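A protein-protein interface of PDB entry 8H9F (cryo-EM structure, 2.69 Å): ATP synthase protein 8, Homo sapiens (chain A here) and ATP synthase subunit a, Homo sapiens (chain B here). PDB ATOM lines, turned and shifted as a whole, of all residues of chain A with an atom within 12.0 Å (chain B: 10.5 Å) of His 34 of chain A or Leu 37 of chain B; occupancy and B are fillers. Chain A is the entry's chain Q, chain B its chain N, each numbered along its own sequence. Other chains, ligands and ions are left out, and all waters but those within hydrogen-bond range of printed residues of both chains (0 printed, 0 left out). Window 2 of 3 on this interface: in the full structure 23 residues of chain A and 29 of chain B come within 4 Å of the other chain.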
ATOM      1  N   MET A  28      11.077 -24.368 -14.670  1.00  0.00           N
ATOM      2  CA  MET A  28      10.973 -24.769 -16.067  1.00  0.00           C
ATOM      3  C   MET A  28      10.274 -23.712 -16.907  1.00  0.00           C
ATOM      4  O   MET A  28      10.563 -23.588 -18.100  1.00  0.00           O
ATOM      5  CB  MET A  28      10.231 -26.098 -16.192  1.00  0.00           C
ATOM      6  CG  MET A  28      11.013 -27.300 -15.717  1.00  0.00           C
ATOM      7  SD  MET A  28      12.557 -27.529 -16.604  1.00  0.00           S
ATOM      8  CE  MET A  28      13.733 -27.135 -15.318  1.00  0.00           C
ATOM      9  N   LEU A  29       9.351 -22.952 -16.314  1.00  0.00           N
ATOM     10  CA  LEU A  29       8.704 -21.874 -17.050  1.00  0.00           C
ATOM     11  C   LEU A  29       9.688 -20.771 -17.410  1.00  0.00           C
ATOM     12  O   LEU A  29       9.509 -20.089 -18.424  1.00  0.00           O
ATOM     13  CB  LEU A  29       7.546 -21.303 -16.238  1.00  0.00           C
ATOM     14  CG  LEU A  29       6.222 -22.051 -16.348  1.00  0.00           C
ATOM     15  CD1 LEU A  29       5.162 -21.338 -15.552  1.00  0.00           C
ATOM     16  CD2 LEU A  29       5.804 -22.177 -17.793  1.00  0.00           C
ATOM     17  N   ASN A  30      10.722 -20.580 -16.600  1.00  0.00           N
ATOM     18  CA  ASN A  30      11.774 -19.621 -16.894  1.00  0.00           C
ATOM     19  C   ASN A  30      12.879 -20.211 -17.755  1.00  0.00           C
ATOM     20  O   ASN A  30      13.935 -19.589 -17.894  1.00  0.00           O
ATOM     21  CB  ASN A  30      12.364 -19.075 -15.595  1.00  0.00           C
ATOM     22  CG  ASN A  30      12.783 -17.627 -15.712  1.00  0.00           C
ATOM     23  OD1 ASN A  30      12.176 -16.851 -16.448  1.00  0.00           O
ATOM     24  ND2 ASN A  30      13.827 -17.253 -14.985  1.00  0.00           N
ATOM     25  N   THR A  31      12.664 -21.393 -18.321  1.00  0.00           N
ATOM     26  CA  THR A  31      13.592 -22.026 -19.252  1.00  0.00           C
ATOM     27  C   THR A  31      12.938 -21.959 -20.624  1.00  0.00           C
ATOM     28  O   THR A  31      12.153 -22.837 -20.989  1.00  0.00           O
ATOM     29  CB  THR A  31      13.894 -23.463 -18.846  1.00  0.00           C
ATOM     30  OG1 THR A  31      14.517 -23.480 -17.558  1.00  0.00           O
ATOM     31  CG2 THR A  31      14.821 -24.117 -19.852  1.00  0.00           C
ATOM     32  N   ASN A  32      13.253 -20.914 -21.379  1.00  0.00           N
ATOM     33  CA  ASN A  32      12.580 -20.635 -22.634  1.00  0.00           C
ATOM     34  C   ASN A  32      13.541 -20.784 -23.803  1.00  0.00           C
ATOM     35  O   ASN A  32      14.734 -20.488 -23.693  1.00  0.00           O
ATOM     36  CB  ASN A  32      11.975 -19.235 -22.631  1.00  0.00           C
ATOM     37  CG  ASN A  32      10.750 -19.139 -21.753  1.00  0.00           C
ATOM     38  OD1 ASN A  32      10.684 -18.313 -20.844  1.00  0.00           O
ATOM     39  ND2 ASN A  32       9.769 -19.993 -22.015  1.00  0.00           N
ATOM     40  N   TYR A  33      13.004 -21.246 -24.925  1.00  0.00           N
ATOM     41  CA  TYR A  33      13.766 -21.471 -26.147  1.00  0.00           C
ATOM     42  C   TYR A  33      13.151 -20.604 -27.237  1.00  0.00           C
ATOM     43  O   TYR A  33      12.114 -20.957 -27.806  1.00  0.00           O
ATOM     44  CB  TYR A  33      13.755 -22.946 -26.529  1.00  0.00           C
ATOM     45  CG  TYR A  33      14.190 -23.848 -25.407  1.00  0.00           C
ATOM     46  CD1 TYR A  33      15.532 -24.046 -25.139  1.00  0.00           C
ATOM     47  CD2 TYR A  33      13.261 -24.493 -24.607  1.00  0.00           C
ATOM     48  CE1 TYR A  33      15.936 -24.861 -24.117  1.00  0.00           C
ATOM     49  CE2 TYR A  33      13.658 -25.310 -23.579  1.00  0.00           C
ATOM     50  CZ  TYR A  33      14.997 -25.490 -23.339  1.00  0.00           C
ATOM     51  OH  TYR A  33      15.410 -26.304 -22.317  1.00  0.00           O
ATOM     52  N   HIS A  34      13.785 -19.471 -27.521  1.00  0.00           N
ATOM     53  CA  HIS A  34      13.262 -18.556 -28.517  1.00  0.00           C
ATOM     54  C   HIS A  34      13.341 -19.181 -29.906  1.00  0.00           C
ATOM     55  O   HIS A  34      13.976 -20.216 -30.124  1.00  0.00           O
ATOM     56  CB  HIS A  34      14.022 -17.231 -28.480  1.00  0.00           C
ATOM     57  CG  HIS A  34      15.472 -17.355 -28.830  1.00  0.00           C
ATOM     58  ND1 HIS A  34      15.922 -17.403 -30.130  1.00  0.00           N
ATOM     59  CD2 HIS A  34      16.573 -17.442 -28.048  1.00  0.00           C
ATOM     60  CE1 HIS A  34      17.238 -17.515 -30.136  1.00  0.00           C
ATOM     61  NE2 HIS A  34      17.657 -17.541 -28.884  1.00  0.00           N
ATOM     62  N   LEU A  35      12.678 -18.540 -30.851  1.00  0.00           N
ATOM     63  CA  LEU A  35      12.672 -19.011 -32.224  1.00  0.00           C
ATOM     64  C   LEU A  35      13.936 -18.537 -32.940  1.00  0.00           C
ATOM     65  O   LEU A  35      14.493 -17.491 -32.601  1.00  0.00           O
ATOM     66  CB  LEU A  35      11.432 -18.503 -32.949  1.00  0.00           C
ATOM     67  CG  LEU A  35      10.155 -19.345 -32.867  1.00  0.00           C
ATOM     68  CD1 LEU A  35       9.819 -19.737 -31.445  1.00  0.00           C
ATOM     69  CD2 LEU A  35       8.993 -18.594 -33.484  1.00  0.00           C
ATOM     70  N   PRO A  36      14.418 -19.291 -33.923  1.00  0.00           N
ATOM     71  CA  PRO A  36      15.691 -18.948 -34.561  1.00  0.00           C
ATOM     72  C   PRO A  36      15.564 -17.684 -35.390  1.00  0.00           C
ATOM     73  O   PRO A  36      14.543 -17.469 -36.058  1.00  0.00           O
ATOM     74  CB  PRO A  36      15.987 -20.168 -35.450  1.00  0.00           C
ATOM     75  CG  PRO A  36      15.022 -21.222 -35.031  1.00  0.00           C
ATOM     76  CD  PRO A  36      13.830 -20.507 -34.504  1.00  0.00           C
ATOM     77  N   PRO A  37      16.576 -16.822 -35.372  1.00  0.00           N
ATOM     78  CA  PRO A  37      16.536 -15.628 -36.217  1.00  0.00           C
ATOM     79  C   PRO A  37      16.768 -15.988 -37.675  1.00  0.00           C
ATOM     80  O   PRO A  37      17.340 -17.029 -38.005  1.00  0.00           O
ATOM     81  CB  PRO A  37      17.675 -14.757 -35.669  1.00  0.00           C
ATOM     82  CG  PRO A  37      18.165 -15.448 -34.424  1.00  0.00           C
ATOM     83  CD  PRO A  37      17.809 -16.884 -34.574  1.00  0.00           C
ATOM     84  N   SER A  38      16.306 -15.102 -38.553  1.00  0.00           N
ATOM     85  CA  SER A  38      16.401 -15.317 -39.996  1.00  0.00           C
ATOM     86  C   SER A  38      17.843 -15.499 -40.459  1.00  0.00           C
ATOM     87  O   SER A  38      18.152 -16.438 -41.191  1.00  0.00           O
ATOM     88  CB  SER A  38      15.760 -14.152 -40.750  1.00  0.00           C
ATOM     89  OG  SER A  38      14.368 -14.094 -40.509  1.00  0.00           O
ATOM     90  N   THR B  33      18.160 -20.413 -13.205  1.00  0.00           N
ATOM     91  CA  THR B  33      17.616 -19.891 -14.446  1.00  0.00           C
ATOM     92  C   THR B  33      18.084 -18.456 -14.643  1.00  0.00           C
ATOM     93  O   THR B  33      18.556 -17.800 -13.712  1.00  0.00           O
ATOM     94  CB  THR B  33      16.086 -19.963 -14.456  1.00  0.00           C
ATOM     95  OG1 THR B  33      15.571 -19.416 -13.238  1.00  0.00           O
ATOM     96  CG2 THR B  33      15.629 -21.400 -14.585  1.00  0.00           C
ATOM     97  N   SER B  34      17.958 -17.975 -15.877  1.00  0.00           N
ATOM     98  CA  SER B  34      18.399 -16.629 -16.206  1.00  0.00           C
ATOM     99  C   SER B  34      17.606 -16.112 -17.393  1.00  0.00           C
ATOM    100  O   SER B  34      17.127 -16.884 -18.226  1.00  0.00           O
ATOM    101  CB  SER B  34      19.898 -16.587 -16.519  1.00  0.00           C
ATOM    102  OG  SER B  34      20.162 -17.070 -17.824  1.00  0.00           O
ATOM    103  N   LYS B  35      17.475 -14.789 -17.456  1.00  0.00           N
ATOM    104  CA  LYS B  35      16.853 -14.117 -18.586  1.00  0.00           C
ATOM    105  C   LYS B  35      17.836 -13.819 -19.707  1.00  0.00           C
ATOM    106  O   LYS B  35      17.406 -13.457 -20.805  1.00  0.00           O
ATOM    107  CB  LYS B  35      16.201 -12.812 -18.125  1.00  0.00           C
ATOM    108  CG  LYS B  35      14.966 -13.002 -17.270  1.00  0.00           C
ATOM    109  CD  LYS B  35      13.830 -13.593 -18.079  1.00  0.00           C
ATOM    110  CE  LYS B  35      12.564 -13.689 -17.251  1.00  0.00           C
ATOM    111  NZ  LYS B  35      12.171 -12.369 -16.696  1.00  0.00           N
ATOM    112  N   TYR B  36      19.135 -13.961 -19.454  1.00  0.00           N
ATOM    113  CA  TYR B  36      20.151 -13.684 -20.455  1.00  0.00           C
ATOM    114  C   TYR B  36      19.916 -14.509 -21.714  1.00  0.00           C
ATOM    115  O   TYR B  36      19.298 -15.575 -21.689  1.00  0.00           O
ATOM    116  CB  TYR B  36      21.542 -13.995 -19.909  1.00  0.00           C
ATOM    117  CG  TYR B  36      22.089 -12.980 -18.938  1.00  0.00           C
ATOM    118  CD1 TYR B  36      23.288 -13.210 -18.277  1.00  0.00           C
ATOM    119  CD2 TYR B  36      21.416 -11.792 -18.681  1.00  0.00           C
ATOM    120  CE1 TYR B  36      23.802 -12.293 -17.387  1.00  0.00           C
ATOM    121  CE2 TYR B  36      21.923 -10.865 -17.789  1.00  0.00           C
ATOM    122  CZ  TYR B  36      23.119 -11.123 -17.146  1.00  0.00           C
ATOM    123  OH  TYR B  36      23.640 -10.212 -16.256  1.00  0.00           O
ATOM    124  N   LEU B  37      20.428 -13.998 -22.830  1.00  0.00           N
ATOM    125  CA  LEU B  37      20.390 -14.752 -24.075  1.00  0.00           C
ATOM    126  C   LEU B  37      21.530 -15.757 -24.136  1.00  0.00           C
ATOM    127  O   LEU B  37      21.354 -16.874 -24.631  1.00  0.00           O
ATOM    128  CB  LEU B  37      20.453 -13.797 -25.264  1.00  0.00           C
ATOM    129  CG  LEU B  37      20.183 -14.382 -26.644  1.00  0.00           C
ATOM    130  CD1 LEU B  37      18.793 -14.973 -26.698  1.00  0.00           C
ATOM    131  CD2 LEU B  37      20.346 -13.305 -27.692  1.00  0.00           C
ATOM    132  N   ILE B  38      22.699 -15.375 -23.631  1.00  0.00           N
ATOM    133  CA  ILE B  38      23.865 -16.245 -23.567  1.00  0.00           C
ATOM    134  C   ILE B  38      24.385 -16.205 -22.140  1.00  0.00           C
ATOM    135  O   ILE B  38      24.694 -15.128 -21.619  1.00  0.00           O
ATOM    136  CB  ILE B  38      24.955 -15.822 -24.562  1.00  0.00           C
ATOM    137  CG1 ILE B  38      24.563 -16.271 -25.968  1.00  0.00           C
ATOM    138  CG2 ILE B  38      26.298 -16.402 -24.161  1.00  0.00           C
ATOM    139  CD1 ILE B  38      25.500 -15.816 -27.031  1.00  0.00           C
ATOM    140  N   ASN B  39      24.473 -17.372 -21.507  1.00  0.00           N
ATOM    141  CA  ASN B  39      24.782 -17.431 -20.087  1.00  0.00           C
ATOM    142  C   ASN B  39      25.804 -18.512 -19.768  1.00  0.00           C
ATOM    143  O   ASN B  39      26.432 -19.068 -20.674  1.00  0.00           O
ATOM    144  CB  ASN B  39      23.494 -17.632 -19.290  1.00  0.00           C
ATOM    145  CG  ASN B  39      22.508 -18.524 -20.002  1.00  0.00           C
ATOM    146  OD1 ASN B  39      22.860 -19.225 -20.949  1.00  0.00           O
ATOM    147  ND2 ASN B  39      21.255 -18.473 -19.579  1.00  0.00           N
ATOM    148  N   ASN B  40      25.971 -18.812 -18.484  1.00  0.00           N
ATOM    149  CA  ASN B  40      27.108 -19.580 -18.004  1.00  0.00           C
ATOM    150  C   ASN B  40      27.044 -21.024 -18.501  1.00  0.00           C
ATOM    151  O   ASN B  40      26.106 -21.443 -19.182  1.00  0.00           O
ATOM    152  CB  ASN B  40      27.165 -19.521 -16.481  1.00  0.00           C
ATOM    153  CG  ASN B  40      25.836 -19.835 -15.836  1.00  0.00           C
ATOM    154  OD1 ASN B  40      25.238 -20.872 -16.099  1.00  0.00           O
ATOM    155  ND2 ASN B  40      25.363 -18.934 -14.990  1.00  0.00           N
ATOM    156  N   ILE B  43      23.958 -23.287 -16.831  1.00  0.00           N
ATOM    157  CA  ILE B  43      22.650 -23.074 -17.436  1.00  0.00           C
ATOM    158  C   ILE B  43      22.643 -23.528 -18.888  1.00  0.00           C
ATOM    159  O   ILE B  43      21.634 -24.042 -19.372  1.00  0.00           O
ATOM    160  CB  ILE B  43      22.236 -21.600 -17.301  1.00  0.00           C
ATOM    161  CG1 ILE B  43      22.031 -21.244 -15.835  1.00  0.00           C
ATOM    162  CG2 ILE B  43      20.965 -21.329 -18.068  1.00  0.00           C
ATOM    163  CD1 ILE B  43      21.480 -19.866 -15.632  1.00  0.00           C
ATOM    164  N   THR B  44      23.757 -23.368 -19.603  1.00  0.00           N
ATOM    165  CA  THR B  44      23.820 -23.826 -20.988  1.00  0.00           C
ATOM    166  C   THR B  44      23.641 -25.337 -21.074  1.00  0.00           C
ATOM    167  O   THR B  44      22.808 -25.837 -21.845  1.00  0.00           O
ATOM    168  CB  THR B  44      25.148 -23.408 -21.614  1.00  0.00           C
ATOM    169  OG1 THR B  44      25.281 -21.986 -21.545  1.00  0.00           O
ATOM    170  CG2 THR B  44      25.211 -23.842 -23.060  1.00  0.00           C
ATOM    171  N   GLN B  47      20.042 -26.310 -20.009  1.00  0.00           N
ATOM    172  CA  GLN B  47      19.027 -26.019 -21.010  1.00  0.00           C
ATOM    173  C   GLN B  47      19.128 -26.977 -22.185  1.00  0.00           C
ATOM    174  O   GLN B  47      18.107 -27.387 -22.744  1.00  0.00           O
ATOM    175  CB  GLN B  47      19.150 -24.574 -21.474  1.00  0.00           C
ATOM    176  CG  GLN B  47      18.610 -23.577 -20.476  1.00  0.00           C
ATOM    177  CD  GLN B  47      18.566 -22.172 -21.023  1.00  0.00           C
ATOM    178  OE1 GLN B  47      17.930 -21.291 -20.448  1.00  0.00           O
ATOM    179  NE2 GLN B  47      19.247 -21.951 -22.138  1.00  0.00           N
ATOM    180  N   LYS B  51      16.064 -29.412 -23.143  1.00  0.00           N
ATOM    181  CA  LYS B  51      15.533 -29.446 -24.500  1.00  0.00           C
ATOM    182  C   LYS B  51      15.561 -30.859 -25.069  1.00  0.00           C
ATOM    183  O   LYS B  51      14.589 -31.305 -25.692  1.00  0.00           O
ATOM    184  CB  LYS B  51      16.325 -28.491 -25.390  1.00  0.00           C
ATOM    185  CG  LYS B  51      15.856 -28.449 -26.828  1.00  0.00           C
ATOM    186  CD  LYS B  51      16.251 -27.148 -27.493  1.00  0.00           C
ATOM    187  CE  LYS B  51      17.740 -26.899 -27.376  1.00  0.00           C
ATOM    188  NZ  LYS B  51      18.524 -27.992 -28.003  1.00  0.00           N
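OD1 of Asn 30 of chain A touches CE of Lys 35 of chain B (3.3 Å). Thr 31 of chain A touches Thr 33 of chain B (OG1 to CG2, 3.8 Å). Thr 31 of chain A touches Gln 47 of chain B. Leu 37 of chain B touches His 34 of chain A.
Hydrophobic or aromatic side chains of chain B that line the printed part of chain A: Leu 37. Among the printed residues, no Asp or Glu carboxylate lies within 4 Å of a Lys or Arg side-chain nitrogen of the other chain.
His 34 of chain A touches one residue of chain B. No residue of chain B comes within 4 Å of Leu 35 of chain A. No residue of chain B comes within 4 Å of Pro 36 of chain A. No residue of chain A comes within 4 Å of Ile 38 of chain B. No residue of chain A comes within 4 Å of Asn 39 of chain B. Of the printed residues of chain A, Lys 51 of chain B touches Tyr 33. Of the printed residues of chain B, Tyr 33 of chain A touches Gln 47 and Lys 51. Leu 29 of chain A touches none of the printed residues of chain B. Asn 32 of chain A touches none of the printed residues of chain B. The nearest printed residue of chain A that does not touch Lys 51 of chain B is Thr 31 of chain A (6.4 Å).
The backbone NH of Lys 51 of chain B lies within hydrogen-bond range of the side-chain hydroxyl of Tyr 33 of chain A (3.3 Å). The backbone carbonyl oxygen (O) of Gln 47 of chain B sits at hydrogen-bond distance from the side-chain hydroxyl (OH) of Tyr 33 of chain A. The side-chain amide nitrogen of Asn 30 of chain A lies within hydrogen-bond range of the side-chain hydroxyl of Thr 33 of chain B (3.3 Å).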
